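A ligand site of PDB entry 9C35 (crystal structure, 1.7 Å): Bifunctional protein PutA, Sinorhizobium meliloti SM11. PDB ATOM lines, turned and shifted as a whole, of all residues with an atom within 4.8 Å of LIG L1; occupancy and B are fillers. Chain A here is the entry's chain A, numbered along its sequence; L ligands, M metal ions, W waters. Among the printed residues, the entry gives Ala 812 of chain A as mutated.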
ATOM      1  N   ILE A 705       0.861  14.697  17.590  1.00  0.00           N
ATOM      2  CA  ILE A 705       1.915  15.492  16.953  1.00  0.00           C
ATOM      3  C   ILE A 705       2.879  15.848  18.056  1.00  0.00           C
ATOM      4  O   ILE A 705       2.453  16.273  19.129  1.00  0.00           O
ATOM      5  CB  ILE A 705       1.348  16.747  16.260  1.00  0.00           C
ATOM      6  CG1 ILE A 705       0.565  16.318  15.017  1.00  0.00           C
ATOM      7  CG2 ILE A 705       2.452  17.718  15.886  1.00  0.00           C
ATOM      8  CD1 ILE A 705      -0.378  17.360  14.512  1.00  0.00           C
ATOM      9  N   SER A 706       4.164  15.632  17.818  1.00  0.00           N
ATOM     10  CA  SER A 706       5.145  15.721  18.907  1.00  0.00           C
ATOM     11  C   SER A 706       6.384  16.508  18.515  1.00  0.00           C
ATOM     12  O   SER A 706       6.642  16.703  17.337  1.00  0.00           O
ATOM     13  CB  SER A 706       5.569  14.309  19.341  1.00  0.00           C
ATOM     14  OG  SER A 706       5.999  13.571  18.196  1.00  0.00           O
ATOM     15  N   PRO A 707       7.133  16.988  19.492  1.00  0.00           N
ATOM     16  CA  PRO A 707       8.268  17.879  19.242  1.00  0.00           C
ATOM     17  C   PRO A 707       9.565  17.073  19.117  1.00  0.00           C
ATOM     18  O   PRO A 707       9.604  15.868  19.380  1.00  0.00           O
ATOM     19  CB  PRO A 707       8.288  18.757  20.509  1.00  0.00           C
ATOM     20  CG  PRO A 707       7.941  17.757  21.575  1.00  0.00           C
ATOM     21  CD  PRO A 707       6.857  16.852  20.937  1.00  0.00           C
ATOM     22  N   TRP A 708      10.617  17.766  18.694  1.00  0.00           N
ATOM     23  CA  TRP A 708      11.897  17.074  18.482  1.00  0.00           C
ATOM     24  C   TRP A 708      12.686  16.856  19.788  1.00  0.00           C
ATOM     25  O   TRP A 708      13.594  16.006  19.801  1.00  0.00           O
ATOM     26  CB  TRP A 708      12.782  17.871  17.503  1.00  0.00           C
ATOM     27  CG  TRP A 708      13.328  19.109  18.165  1.00  0.00           C
ATOM     28  CD1 TRP A 708      12.836  20.372  18.080  1.00  0.00           C
ATOM     29  CD2 TRP A 708      14.472  19.177  19.033  1.00  0.00           C
ATOM     30  NE1 TRP A 708      13.596  21.224  18.866  1.00  0.00           N
ATOM     31  CE2 TRP A 708      14.603  20.510  19.455  1.00  0.00           C
ATOM     32  CE3 TRP A 708      15.403  18.229  19.487  1.00  0.00           C
ATOM     33  CZ2 TRP A 708      15.637  20.931  20.312  1.00  0.00           C
ATOM     34  CZ3 TRP A 708      16.424  18.644  20.362  1.00  0.00           C
ATOM     35  CH2 TRP A 708      16.524  19.989  20.760  1.00  0.00           C
ATOM     36  N   ASN A 709      12.387  17.602  20.846  1.00  0.00           N
ATOM     37  CA  ASN A 709      13.324  17.707  21.972  1.00  0.00           C
ATOM     38  C   ASN A 709      13.135  16.637  23.040  1.00  0.00           C
ATOM     39  O   ASN A 709      14.018  16.446  23.873  1.00  0.00           O
ATOM     40  CB  ASN A 709      13.194  19.088  22.634  1.00  0.00           C
ATOM     41  CG  ASN A 709      11.928  19.222  23.457  1.00  0.00           C
ATOM     42  OD1 ASN A 709      10.831  19.037  22.961  1.00  0.00           O
ATOM     43  ND2 ASN A 709      12.103  19.518  24.742  1.00  0.00           N
ATOM     44  N   PHE A 710      12.004  15.943  23.030  1.00  0.00           N
ATOM     45  CA  PHE A 710      11.832  14.692  23.764  1.00  0.00           C
ATOM     46  C   PHE A 710      11.276  13.711  22.744  1.00  0.00           C
ATOM     47  O   PHE A 710      10.087  13.368  22.770  1.00  0.00           O
ATOM     48  CB  PHE A 710      10.936  14.851  24.992  1.00  0.00           C
ATOM     49  CG  PHE A 710      11.616  15.602  26.095  1.00  0.00           C
ATOM     50  CD1 PHE A 710      12.508  14.968  26.919  1.00  0.00           C
ATOM     51  CD2 PHE A 710      11.389  16.960  26.293  1.00  0.00           C
ATOM     52  CE1 PHE A 710      13.169  15.651  27.924  1.00  0.00           C
ATOM     53  CE2 PHE A 710      12.049  17.643  27.298  1.00  0.00           C
ATOM     54  CZ  PHE A 710      12.944  16.980  28.103  1.00  0.00           C
ATOM     55  N   ILE A 714       7.897  12.082  25.005  1.00  0.00           N
ATOM     56  CA  ILE A 714       6.605  12.725  24.803  1.00  0.00           C
ATOM     57  C   ILE A 714       5.873  12.040  23.647  1.00  0.00           C
ATOM     58  O   ILE A 714       4.654  11.814  23.718  1.00  0.00           O
ATOM     59  CB  ILE A 714       6.785  14.235  24.573  1.00  0.00           C
ATOM     60  CG1 ILE A 714       7.184  14.881  25.920  1.00  0.00           C
ATOM     61  CG2 ILE A 714       5.504  14.875  24.006  1.00  0.00           C
ATOM     62  CD1 ILE A 714       7.658  16.295  25.840  1.00  0.00           C
ATOM     63  N   LYS A 732       2.526  11.521  14.228  1.00  0.00           N
ATOM     64  CA  LYS A 732       3.287  12.418  13.360  1.00  0.00           C
ATOM     65  C   LYS A 732       4.486  12.961  14.141  1.00  0.00           C
ATOM     66  O   LYS A 732       4.338  13.879  14.932  1.00  0.00           O
ATOM     67  CB  LYS A 732       2.402  13.558  12.848  1.00  0.00           C
ATOM     68  CG  LYS A 732       2.709  13.972  11.398  1.00  0.00           C
ATOM     69  CD  LYS A 732       4.126  14.570  11.277  1.00  0.00           C
ATOM     70  CE  LYS A 732       4.238  15.921  11.963  1.00  0.00           C
ATOM     71  NZ  LYS A 732       5.546  16.582  11.735  1.00  0.00           N
ATOM     72  N   PRO A 733       5.694  12.420  13.951  1.00  0.00           N
ATOM     73  CA  PRO A 733       6.845  12.883  14.728  1.00  0.00           C
ATOM     74  C   PRO A 733       7.409  14.169  14.132  1.00  0.00           C
ATOM     75  O   PRO A 733       7.277  14.438  12.950  1.00  0.00           O
ATOM     76  CB  PRO A 733       7.850  11.737  14.604  1.00  0.00           C
ATOM     77  CG  PRO A 733       7.533  11.107  13.274  1.00  0.00           C
ATOM     78  CD  PRO A 733       5.995  11.282  13.098  1.00  0.00           C
ATOM     79  N   ALA A 734       8.089  14.929  14.973  1.00  0.00           N
ATOM     80  CA  ALA A 734       8.786  16.101  14.454  1.00  0.00           C
ATOM     81  C   ALA A 734       9.686  15.692  13.293  1.00  0.00           C
ATOM     82  O   ALA A 734      10.242  14.596  13.246  1.00  0.00           O
ATOM     83  CB  ALA A 734       9.631  16.758  15.546  1.00  0.00           C
ATOM     84  N   GLU A 735       9.857  16.618  12.345  1.00  0.00           N
ATOM     85  CA  GLU A 735      10.615  16.295  11.147  1.00  0.00           C
ATOM     86  C   GLU A 735      12.097  16.093  11.439  1.00  0.00           C
ATOM     87  O   GLU A 735      12.799  15.446  10.649  1.00  0.00           O
ATOM     88  CB  GLU A 735      10.422  17.370  10.080  1.00  0.00           C
ATOM     89  CG  GLU A 735      10.745  18.793  10.496  1.00  0.00           C
ATOM     90  CD  GLU A 735       9.538  19.529  11.095  1.00  0.00           C
ATOM     91  OE1 GLU A 735       8.633  18.867  11.658  1.00  0.00           O
ATOM     92  OE2 GLU A 735       9.510  20.783  11.014  1.00  0.00           O
ATOM     93  N   GLU A 736      12.590  16.616  12.568  1.00  0.00           N
ATOM     94  CA  GLU A 736      14.003  16.455  12.871  1.00  0.00           C
ATOM     95  C   GLU A 736      14.350  15.101  13.497  1.00  0.00           C
ATOM     96  O   GLU A 736      15.511  14.673  13.408  1.00  0.00           O
ATOM     97  CB  GLU A 736      14.460  17.588  13.810  1.00  0.00           C
ATOM     98  CG  GLU A 736      14.297  18.988  13.220  1.00  0.00           C
ATOM     99  CD  GLU A 736      12.999  19.708  13.666  1.00  0.00           C
ATOM    100  OE1 GLU A 736      12.026  19.042  14.113  1.00  0.00           O
ATOM    101  OE2 GLU A 736      12.961  20.971  13.564  1.00  0.00           O
ATOM    102  N   GLY A 763       7.351  13.344   8.524  1.00  0.00           N
ATOM    103  CA  GLY A 763       7.209  14.538   7.717  1.00  0.00           C
ATOM    104  C   GLY A 763       7.101  15.821   8.515  1.00  0.00           C
ATOM    105  O   GLY A 763       7.185  15.836   9.752  1.00  0.00           O
ATOM    106  N   ASP A 764       6.901  16.928   7.809  1.00  0.00           N
ATOM    107  CA  ASP A 764       6.956  18.243   8.409  1.00  0.00           C
ATOM    108  C   ASP A 764       5.551  18.714   8.800  1.00  0.00           C
ATOM    109  O   ASP A 764       4.618  17.910   8.897  1.00  0.00           O
ATOM    110  CB  ASP A 764       7.625  19.227   7.443  1.00  0.00           C
ATOM    111  CG  ASP A 764       6.966  19.244   6.071  1.00  0.00           C
ATOM    112  OD1 ASP A 764       5.731  19.408   6.006  1.00  0.00           O
ATOM    113  OD2 ASP A 764       7.689  19.050   5.072  1.00  0.00           O
ATOM    114  N   GLY A 765       5.398  20.013   9.025  1.00  0.00           N
ATOM    115  CA  GLY A 765       4.115  20.537   9.479  1.00  0.00           C
ATOM    116  C   GLY A 765       2.971  20.317   8.510  1.00  0.00           C
ATOM    117  O   GLY A 765       1.803  20.286   8.929  1.00  0.00           O
ATOM    118  N   GLY A 768       1.413  17.115   9.455  1.00  0.00           N
ATOM    119  CA  GLY A 768       0.616  17.351  10.648  1.00  0.00           C
ATOM    120  C   GLY A 768      -0.675  18.103  10.348  1.00  0.00           C
ATOM    121  O   GLY A 768      -1.720  17.787  10.900  1.00  0.00           O
ATOM    122  N   ALA A 769      -0.603  19.086   9.451  1.00  0.00           N
ATOM    123  CA  ALA A 769      -1.783  19.898   9.180  1.00  0.00           C
ATOM    124  C   ALA A 769      -2.826  19.102   8.391  1.00  0.00           C
ATOM    125  O   ALA A 769      -4.032  19.311   8.570  1.00  0.00           O
ATOM    126  CB  ALA A 769      -1.383  21.166   8.425  1.00  0.00           C
ATOM    127  N   PHE A 782      -1.275  17.562  20.894  1.00  0.00           N
ATOM    128  CA  PHE A 782      -0.202  18.383  20.352  1.00  0.00           C
ATOM    129  C   PHE A 782       0.732  18.721  21.485  1.00  0.00           C
ATOM    130  O   PHE A 782       0.283  19.108  22.552  1.00  0.00           O
ATOM    131  CB  PHE A 782      -0.731  19.692  19.704  1.00  0.00           C
ATOM    132  CG  PHE A 782       0.371  20.595  19.199  1.00  0.00           C
ATOM    133  CD1 PHE A 782       1.046  20.328  18.006  1.00  0.00           C
ATOM    134  CD2 PHE A 782       0.766  21.690  19.951  1.00  0.00           C
ATOM    135  CE1 PHE A 782       2.092  21.141  17.550  1.00  0.00           C
ATOM    136  CE2 PHE A 782       1.814  22.504  19.509  1.00  0.00           C
ATOM    137  CZ  PHE A 782       2.476  22.236  18.312  1.00  0.00           C
ATOM    138  N   THR A 783       2.026  18.532  21.279  1.00  0.00           N
ATOM    139  CA  THR A 783       3.061  19.139  22.124  1.00  0.00           C
ATOM    140  C   THR A 783       4.040  19.826  21.180  1.00  0.00           C
ATOM    141  O   THR A 783       4.500  19.209  20.220  1.00  0.00           O
ATOM    142  CB  THR A 783       3.751  18.067  22.990  1.00  0.00           C
ATOM    143  OG1 THR A 783       2.766  17.404  23.803  1.00  0.00           O
ATOM    144  CG2 THR A 783       4.829  18.735  23.886  1.00  0.00           C
ATOM    145  N   GLY A 784       4.352  21.086  21.461  1.00  0.00           N
ATOM    146  CA  GLY A 784       5.075  21.920  20.506  1.00  0.00           C
ATOM    147  C   GLY A 784       4.955  23.387  20.910  1.00  0.00           C
ATOM    148  O   GLY A 784       4.633  23.712  22.051  1.00  0.00           O
ATOM    149  N   SER A 785       5.203  24.255  19.929  1.00  0.00           N
ATOM    150  CA  SER A 785       5.208  25.682  20.165  1.00  0.00           C
ATOM    151  C   SER A 785       3.794  26.235  20.340  1.00  0.00           C
ATOM    152  O   SER A 785       2.807  25.677  19.842  1.00  0.00           O
ATOM    153  CB  SER A 785       5.909  26.393  19.001  1.00  0.00           C
ATOM    154  OG  SER A 785       5.235  26.209  17.762  1.00  0.00           O
ATOM    155  N   VAL A 788       2.086  27.315  16.879  1.00  0.00           N
ATOM    156  CA  VAL A 788       1.605  26.210  16.051  1.00  0.00           C
ATOM    157  C   VAL A 788       0.333  25.634  16.648  1.00  0.00           C
ATOM    158  O   VAL A 788      -0.617  25.320  15.930  1.00  0.00           O
ATOM    159  CB  VAL A 788       2.701  25.156  15.863  1.00  0.00           C
ATOM    160  CG1 VAL A 788       2.154  23.921  15.179  1.00  0.00           C
ATOM    161  CG2 VAL A 788       3.802  25.757  15.061  1.00  0.00           C
ATOM    162  N   LEU A 791      -2.409  27.618  15.389  1.00  0.00           N
ATOM    163  CA  LEU A 791      -2.833  27.295  14.029  1.00  0.00           C
ATOM    164  C   LEU A 791      -3.702  26.034  13.997  1.00  0.00           C
ATOM    165  O   LEU A 791      -4.640  25.941  13.197  1.00  0.00           O
ATOM    166  CB  LEU A 791      -1.604  27.134  13.144  1.00  0.00           C
ATOM    167  CG  LEU A 791      -0.791  28.388  12.840  1.00  0.00           C
ATOM    168  CD1 LEU A 791       0.497  27.998  12.146  1.00  0.00           C
ATOM    169  CD2 LEU A 791      -1.582  29.348  11.962  1.00  0.00           C
ATOM    170  N   ILE A 792      -3.408  25.065  14.865  1.00  0.00           N
ATOM    171  CA  ILE A 792      -4.241  23.861  14.929  1.00  0.00           C
ATOM    172  C   ILE A 792      -5.621  24.204  15.509  1.00  0.00           C
ATOM    173  O   ILE A 792      -6.662  23.783  14.981  1.00  0.00           O
ATOM    174  CB  ILE A 792      -3.518  22.765  15.725  1.00  0.00           C
ATOM    175  CG1 ILE A 792      -2.351  22.242  14.903  1.00  0.00           C
ATOM    176  CG2 ILE A 792      -4.466  21.619  16.105  1.00  0.00           C
ATOM    177  CD1 ILE A 792      -1.271  21.588  15.732  1.00  0.00           C
ATOM    178  N   GLN A 795      -7.684  25.594  12.732  1.00  0.00           N
ATOM    179  CA  GLN A 795      -8.167  24.516  11.874  1.00  0.00           C
ATOM    180  C   GLN A 795      -9.381  23.835  12.476  1.00  0.00           C
ATOM    181  O   GLN A 795     -10.340  23.481  11.778  1.00  0.00           O
ATOM    182  CB  GLN A 795      -7.086  23.455  11.690  1.00  0.00           C
ATOM    183  CG  GLN A 795      -6.370  23.406  10.394  1.00  0.00           C
ATOM    184  CD  GLN A 795      -5.227  22.373  10.426  1.00  0.00           C
ATOM    185  OE1 GLN A 795      -4.618  22.134  11.482  1.00  0.00           O
ATOM    186  NE2 GLN A 795      -4.940  21.748   9.286  1.00  0.00           N
ATOM    187  N   ALA A 812       0.110  21.057  24.787  1.00  0.00           N
ATOM    188  CA  ALA A 812       1.167  21.264  25.776  1.00  0.00           C
ATOM    189  C   ALA A 812       2.217  22.160  25.108  1.00  0.00           C
ATOM    190  O   ALA A 812       2.896  21.727  24.185  1.00  0.00           O
ATOM    191  CB  ALA A 812       1.762  19.928  26.202  1.00  0.00           C
ATOM    192  N   THR A 813       2.360  23.399  25.580  1.00  0.00           N
ATOM    193  CA  THR A 813       3.128  24.362  24.806  1.00  0.00           C
ATOM    194  C   THR A 813       4.246  24.994  25.639  1.00  0.00           C
ATOM    195  O   THR A 813       4.698  24.424  26.623  1.00  0.00           O
ATOM    196  CB  THR A 813       2.184  25.412  24.185  1.00  0.00           C
ATOM    197  OG1 THR A 813       1.270  25.928  25.157  1.00  0.00           O
ATOM    198  CG2 THR A 813       1.370  24.779  23.056  1.00  0.00           C
ATOM    199  N   GLY A 814       4.722  26.144  25.213  1.00  0.00           N
ATOM    200  CA  GLY A 814       5.980  26.662  25.722  1.00  0.00           C
ATOM    201  C   GLY A 814       5.933  27.228  27.122  1.00  0.00           C
ATOM    202  O   GLY A 814       4.891  27.288  27.788  1.00  0.00           O
ATOM    203  N   GLY A 815       7.090  27.713  27.561  1.00  0.00           N
ATOM    204  CA  GLY A 815       7.223  28.287  28.885  1.00  0.00           C
ATOM    205  C   GLY A 815       8.180  29.472  28.862  1.00  0.00           C
ATOM    206  O   GLY A 815       8.879  29.712  27.876  1.00  0.00           O
ATOM    207  N   CYS A 846      11.231  22.392  27.427  1.00  0.00           N
ATOM    208  CA  CYS A 846      10.176  23.357  27.688  1.00  0.00           C
ATOM    209  C   CYS A 846      10.234  23.851  29.137  1.00  0.00           C
ATOM    210  O   CYS A 846       9.791  24.960  29.413  1.00  0.00           O
ATOM    211  CB  CYS A 846       8.810  22.743  27.371  1.00  0.00           C
ATOM    212  SG  CYS A 846       8.516  21.241  28.264  1.00  0.00           S
ATOM    213  N   GLU A 942       9.634  33.155  24.173  1.00  0.00           N
ATOM    214  CA  GLU A 942      10.422  31.996  24.577  1.00  0.00           C
ATOM    215  C   GLU A 942      11.636  31.860  23.656  1.00  0.00           C
ATOM    216  O   GLU A 942      11.482  31.821  22.436  1.00  0.00           O
ATOM    217  CB  GLU A 942       9.573  30.735  24.526  1.00  0.00           C
ATOM    218  CG  GLU A 942      10.293  29.458  25.007  1.00  0.00           C
ATOM    219  CD  GLU A 942       9.573  28.150  24.686  1.00  0.00           C
ATOM    220  OE1 GLU A 942       9.149  27.934  23.519  1.00  0.00           O
ATOM    221  OE2 GLU A 942       9.425  27.330  25.612  1.00  0.00           O
ATOM    222  N   PHE A 944      14.396  29.293  22.790  1.00  0.00           N
ATOM    223  CA  PHE A 944      14.541  27.859  23.023  1.00  0.00           C
ATOM    224  C   PHE A 944      15.994  27.464  22.803  1.00  0.00           C
ATOM    225  O   PHE A 944      16.369  26.853  21.803  1.00  0.00           O
ATOM    226  CB  PHE A 944      13.585  27.059  22.129  1.00  0.00           C
ATOM    227  CG  PHE A 944      13.173  25.732  22.733  1.00  0.00           C
ATOM    228  CD1 PHE A 944      12.395  25.693  23.883  1.00  0.00           C
ATOM    229  CD2 PHE A 944      13.553  24.535  22.152  1.00  0.00           C
ATOM    230  CE1 PHE A 944      12.031  24.484  24.428  1.00  0.00           C
ATOM    231  CE2 PHE A 944      13.167  23.306  22.704  1.00  0.00           C
ATOM    232  CZ  PHE A 944      12.417  23.299  23.845  1.00  0.00           C
ATOM    233  N   LEU A 972       4.338  27.352  33.072  1.00  0.00           N
ATOM    234  CA  LEU A 972       4.762  25.963  33.045  1.00  0.00           C
ATOM    235  C   LEU A 972       5.543  25.583  34.304  1.00  0.00           C
ATOM    236  O   LEU A 972       4.940  25.036  35.256  1.00  0.00           O
ATOM    237  CB  LEU A 972       5.573  25.688  31.781  1.00  0.00           C
ATOM    238  CG  LEU A 972       5.988  24.269  31.440  1.00  0.00           C
ATOM    239  CD1 LEU A 972       4.838  23.290  31.469  1.00  0.00           C
ATOM    240  CD2 LEU A 972       6.611  24.208  30.042  1.00  0.00           C
ATOM    241  N   PHE A1012       2.968  16.522  34.771  1.00  0.00           N
ATOM    242  CA  PHE A1012       3.565  17.648  34.090  1.00  0.00           C
ATOM    243  C   PHE A1012       2.611  18.383  33.161  1.00  0.00           C
ATOM    244  O   PHE A1012       1.949  17.780  32.293  1.00  0.00           O
ATOM    245  CB  PHE A1012       4.816  17.223  33.291  1.00  0.00           C
ATOM    246  CG  PHE A1012       5.577  18.371  32.747  1.00  0.00           C
ATOM    247  CD1 PHE A1012       6.409  19.113  33.586  1.00  0.00           C
ATOM    248  CD2 PHE A1012       5.446  18.754  31.445  1.00  0.00           C
ATOM    249  CE1 PHE A1012       7.077  20.199  33.126  1.00  0.00           C
ATOM    250  CE2 PHE A1012       6.132  19.858  30.964  1.00  0.00           C
ATOM    251  CZ  PHE A1012       6.960  20.588  31.820  1.00  0.00           C
ATOM    252  N   SER A1018       1.059  28.182  28.256  1.00  0.00           N
ATOM    253  CA  SER A1018       1.823  26.954  28.316  1.00  0.00           C
ATOM    254  C   SER A1018       0.972  25.706  28.126  1.00  0.00           C
ATOM    255  O   SER A1018       1.526  24.618  28.035  1.00  0.00           O
ATOM    256  CB  SER A1018       2.557  26.832  29.660  1.00  0.00           C
ATOM    257  OG  SER A1018       3.354  27.973  29.901  1.00  0.00           O
HETATM  258  P1  LIG L   1       7.005  23.064  16.836  1.00  0.00           P
HETATM  259  O1  LIG L   1       5.744  23.892  17.191  1.00  0.00           O
HETATM  260  O2  LIG L   1       7.973  23.715  15.963  1.00  0.00           O
HETATM  261  O3  LIG L   1       6.791  21.796  16.084  1.00  0.00           O
HETATM  262  C1  LIG L   1       6.040  20.783  16.707  1.00  0.00           C
HETATM  263  C2  LIG L   1       5.303  19.771  15.846  1.00  0.00           C
HETATM  264  O4  LIG L   1       4.170  20.300  15.142  1.00  0.00           O
HETATM  265  C3  LIG L   1       6.126  19.036  14.805  1.00  0.00           C
HETATM  266  O5  LIG L   1       5.767  17.695  14.753  1.00  0.00           O
HETATM  267  C4  LIG L   1       5.828  19.783  13.546  1.00  0.00           C
HETATM  268  O6  LIG L   1       6.125  18.977  12.473  1.00  0.00           O
HETATM  269  C5  LIG L   1       4.400  20.086  13.748  1.00  0.00           C
HETATM  270  N1  LIG L   1       3.880  21.236  13.070  1.00  0.00           N
HETATM  271  C6  LIG L   1       4.495  22.397  12.672  1.00  0.00           C
HETATM  272  N2  LIG L   1       3.614  23.188  12.078  1.00  0.00           N
HETATM  273  C7  LIG L   1       2.381  22.577  12.074  1.00  0.00           C
HETATM  274  C8  LIG L   1       1.131  22.901  11.611  1.00  0.00           C
HETATM  275  N3  LIG L   1       0.859  24.150  10.958  1.00  0.00           N
HETATM  276  N4  LIG L   1       0.137  22.032  11.786  1.00  0.00           N
HETATM  277  C9  LIG L   1       0.295  20.838  12.400  1.00  0.00           C
HETATM  278  N5  LIG L   1       1.502  20.480  12.867  1.00  0.00           N
HETATM  279  C10 LIG L   1       2.532  21.325  12.710  1.00  0.00           C
HETATM  280  O7  LIG L   1       7.796  22.653  18.052  1.00  0.00           O
HETATM  281  P2  LIG L   1       9.261  22.083  18.268  1.00  0.00           P
HETATM  282  O8  LIG L   1      10.200  23.107  17.683  1.00  0.00           O
HETATM  283  O9  LIG L   1       9.388  20.677  17.747  1.00  0.00           O
HETATM  284  O10 LIG L   1       9.488  21.957  19.822  1.00  0.00           O
HETATM  285  C11 LIG L   1       9.756  23.087  20.606  1.00  0.00           C
HETATM  286  C12 LIG L   1       8.523  23.693  21.296  1.00  0.00           C
HETATM  287  O11 LIG L   1       7.725  22.716  21.932  1.00  0.00           O
HETATM  288  C13 LIG L   1       8.947  24.707  22.318  1.00  0.00           C
HETATM  289  O12 LIG L   1       8.184  25.850  22.289  1.00  0.00           O
HETATM  290  C14 LIG L   1       8.775  23.956  23.577  1.00  0.00           C
HETATM  291  O13 LIG L   1       8.625  24.745  24.686  1.00  0.00           O
HETATM  292  C15 LIG L   1       7.570  23.115  23.270  1.00  0.00           C
HETATM  293  N6  LIG L   1       7.482  21.984  24.163  1.00  0.00           N
HETATM  294  C16 LIG L   1       6.480  21.940  25.172  1.00  0.00           C
HETATM  295  C17 LIG L   1       6.411  20.837  26.015  1.00  0.00           C
HETATM  296  C18 LIG L   1       5.380  20.707  27.083  1.00  0.00           C
HETATM  297  O14 LIG L   1       5.257  19.619  27.666  1.00  0.00           O
HETATM  298  N7  LIG L   1       4.517  21.793  27.443  1.00  0.00           N
HETATM  299  C19 LIG L   1       7.364  19.783  25.879  1.00  0.00           C
HETATM  300  C20 LIG L   1       8.350  19.856  24.884  1.00  0.00           C
HETATM  301  C21 LIG L   1       8.408  20.945  24.031  1.00  0.00           C
HETATM  302  N1  LG2 L   2       8.794  17.301  31.157  1.00  0.00           N
HETATM  303  C1  LG2 L   2      10.187  17.515  30.824  1.00  0.00           C
HETATM  304  C2  LG2 L   2      10.999  18.030  32.009  1.00  0.00           C
HETATM  305  C3  LG2 L   2      10.332  18.668  29.837  1.00  0.00           C
HETATM  306  C4  LG2 L   2       9.296  18.552  28.718  1.00  0.00           C
HETATM  307  C5  LG2 L   2       9.482  19.828  27.907  1.00  0.00           C
HETATM  308  O1  LG2 L   2      10.303  19.985  27.041  1.00  0.00           O
HETATM  309  O2  LG2 L   2      10.365  18.285  33.057  1.00  0.00           O
HETATM  310  O3  LG2 L   2      12.238  18.215  31.916  1.00  0.00           O
HETATM  311 MG    MG M   1       9.837  23.679  13.659  1.00  0.00          MG
HETATM  312  O   HOH W   1       5.925  28.387  22.652  1.00  0.00           O
HETATM  313  O   HOH W   2      -2.225  23.182  11.515  1.00  0.00           O
HETATM  314  O   HOH W   3       8.475  21.759  13.238  1.00  0.00           O
HETATM  315  O   HOH W   4       7.692  24.116  12.955  1.00  0.00           O
HETATM  316  O   HOH W   5      10.805  22.711  15.255  1.00  0.00           O
HETATM  317  O   HOH W   6       3.793  17.477  28.393  1.00  0.00           O
HETATM  318  O   HOH W   7       1.770  22.398  29.371  1.00  0.00           O
HETATM  319  O   HOH W   8       9.498  19.941  14.542  1.00  0.00           O
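The side-chain hydroxyl of Ser 785 lies within hydrogen-bond range of an oxygen (O1) of LIG L1 (2.4 Å). The side-chain carboxylate (OE1) of Glu 942 lies within hydrogen-bond range of an oxygen (O12) of LIG L1. A carbon (C5) of LG2 L2 is covalently linked to the side-chain sulfur (SG) of Cys 846. N of Ser 785 sits at hydrogen-bond distance from O1 of LIG L1 (2.8 Å). The side-chain amino group of Lys 732 is in hydrogen-bond range of an oxygen (O6) of LIG L1. An oxygen (O5) of LIG L1 lies within hydrogen-bond range of the backbone carbonyl oxygen (O) of Ser 706, at 2.9 Å. An oxygen (O6) of LIG L1 sits at hydrogen-bond distance from the side-chain carboxylate of Glu 735 (2.6 Å). N of Trp 708 is in hydrogen-bond range of O9 of LIG L1 (3.3 Å). N of Cys 846 lies within hydrogen-bond range of O1 of LG2 L2. O1 of LG2 L2 is in hydrogen-bond range of ND2 of Asn 709 (3.0 Å). A nitrogen (N7) of LIG L1 lies within hydrogen-bond range of the backbone carbonyl oxygen of Thr 813 (2.8 Å).
The side-chain amino group (NZ) of Lys 732 sits at hydrogen-bond distance from the backbone carbonyl oxygen (O) of Asp 764. OG of Ser 785 lies close to N of Val 788, 3.5 Å away. NZ of Lys 732 is in hydrogen-bond range of O of Gly 763, 2.7 Å away. The backbone carbonyl oxygen of Ala 769 sits at hydrogen-bond distance from the side-chain amide nitrogen of Gln 795, at 2.7 Å. O of Ile 705 lies within hydrogen-bond range of N of Thr 783, at 3.1 Å. The backbone carbonyl oxygen (O) of Ser 706 is in hydrogen-bond range of the backbone NH (N) of Ala 734. The backbone NH (N) of Gly 815 is in hydrogen-bond range of the side-chain carboxylate (OE2) of Glu 942, at 3.1 Å. NZ of Lys 732 lies within salt-bridge range of OE1 of Glu 735, at 3.8 Å.
O of Gly 784 lies close to O11 of LIG L1 (3.3 Å). The side-chain sulfur (SG) of Cys 846 lies close to an oxygen (O14) of LIG L1 (3.7 Å). Residues that only touch LIG L1: Ile 705, Pro 707, Asn 709, Ile 714, Pro 733, Ala 734, Asp 764, Gly 765, Gly 768, Ala 769, Phe 782, Thr 783, Val 788, Ile 792, Ala 812, Gly 814, Phe 944 and Phe 1012. Hydrophobic or aromatic side chains that line LIG L1: Ile 705, Pro 707, Trp 708, Ile 714, Ala 769, Phe 782, Val 788, Ile 792, Ala 812, Phe 944 and Phe 1012. Within 4 Å of LIG L1: Ile 705, Ser 706, Pro 707, Trp 708, Asn 709, Ile 714, Lys 732, Pro 733, Ala 734, Glu 735, Asp 764, Gly 765, Gly 768, Ala 769, Phe 782, Thr 783, Gly 784, Ser 785, Val 788, Ile 792, Ala 812, Thr 813, Gly 814, Cys 846, Glu 942, Phe 944 and Phe 1012. The nearest printed residue that does not touch LIG L1 is Leu 791 (4.04 Å).
Water W5 lies within hydrogen-bond range of O8 of LIG L1 (2.5 Å) and OE2 of Glu 736 (3.2 Å). Water W2 lies within hydrogen-bond range of the side-chain amide oxygen (OE1) of Gln 795 (2.6 Å) and a nitrogen (N4) of LIG L1 (2.6 Å). Water W8 lies within hydrogen-bond range of the side-chain carboxylate of Glu 736 (2.7 Å), the side-chain carboxylate of Glu 735 (3.2 Å) and an oxygen (O9) of LIG L1 (3.3 Å). Water W3 bridges the side-chain carboxylate of Glu 735 (2.6 Å) and an oxygen (O3) of LIG L1 (3.3 Å). Water W7 lies within hydrogen-bond range of the backbone carbonyl oxygen of Ser 1018 (2.6 Å) and a nitrogen (N7) of LIG L1 (3.4 Å). Water W1 lies within hydrogen-bond range of OE1 of Glu 942 and O12 of LIG L1.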
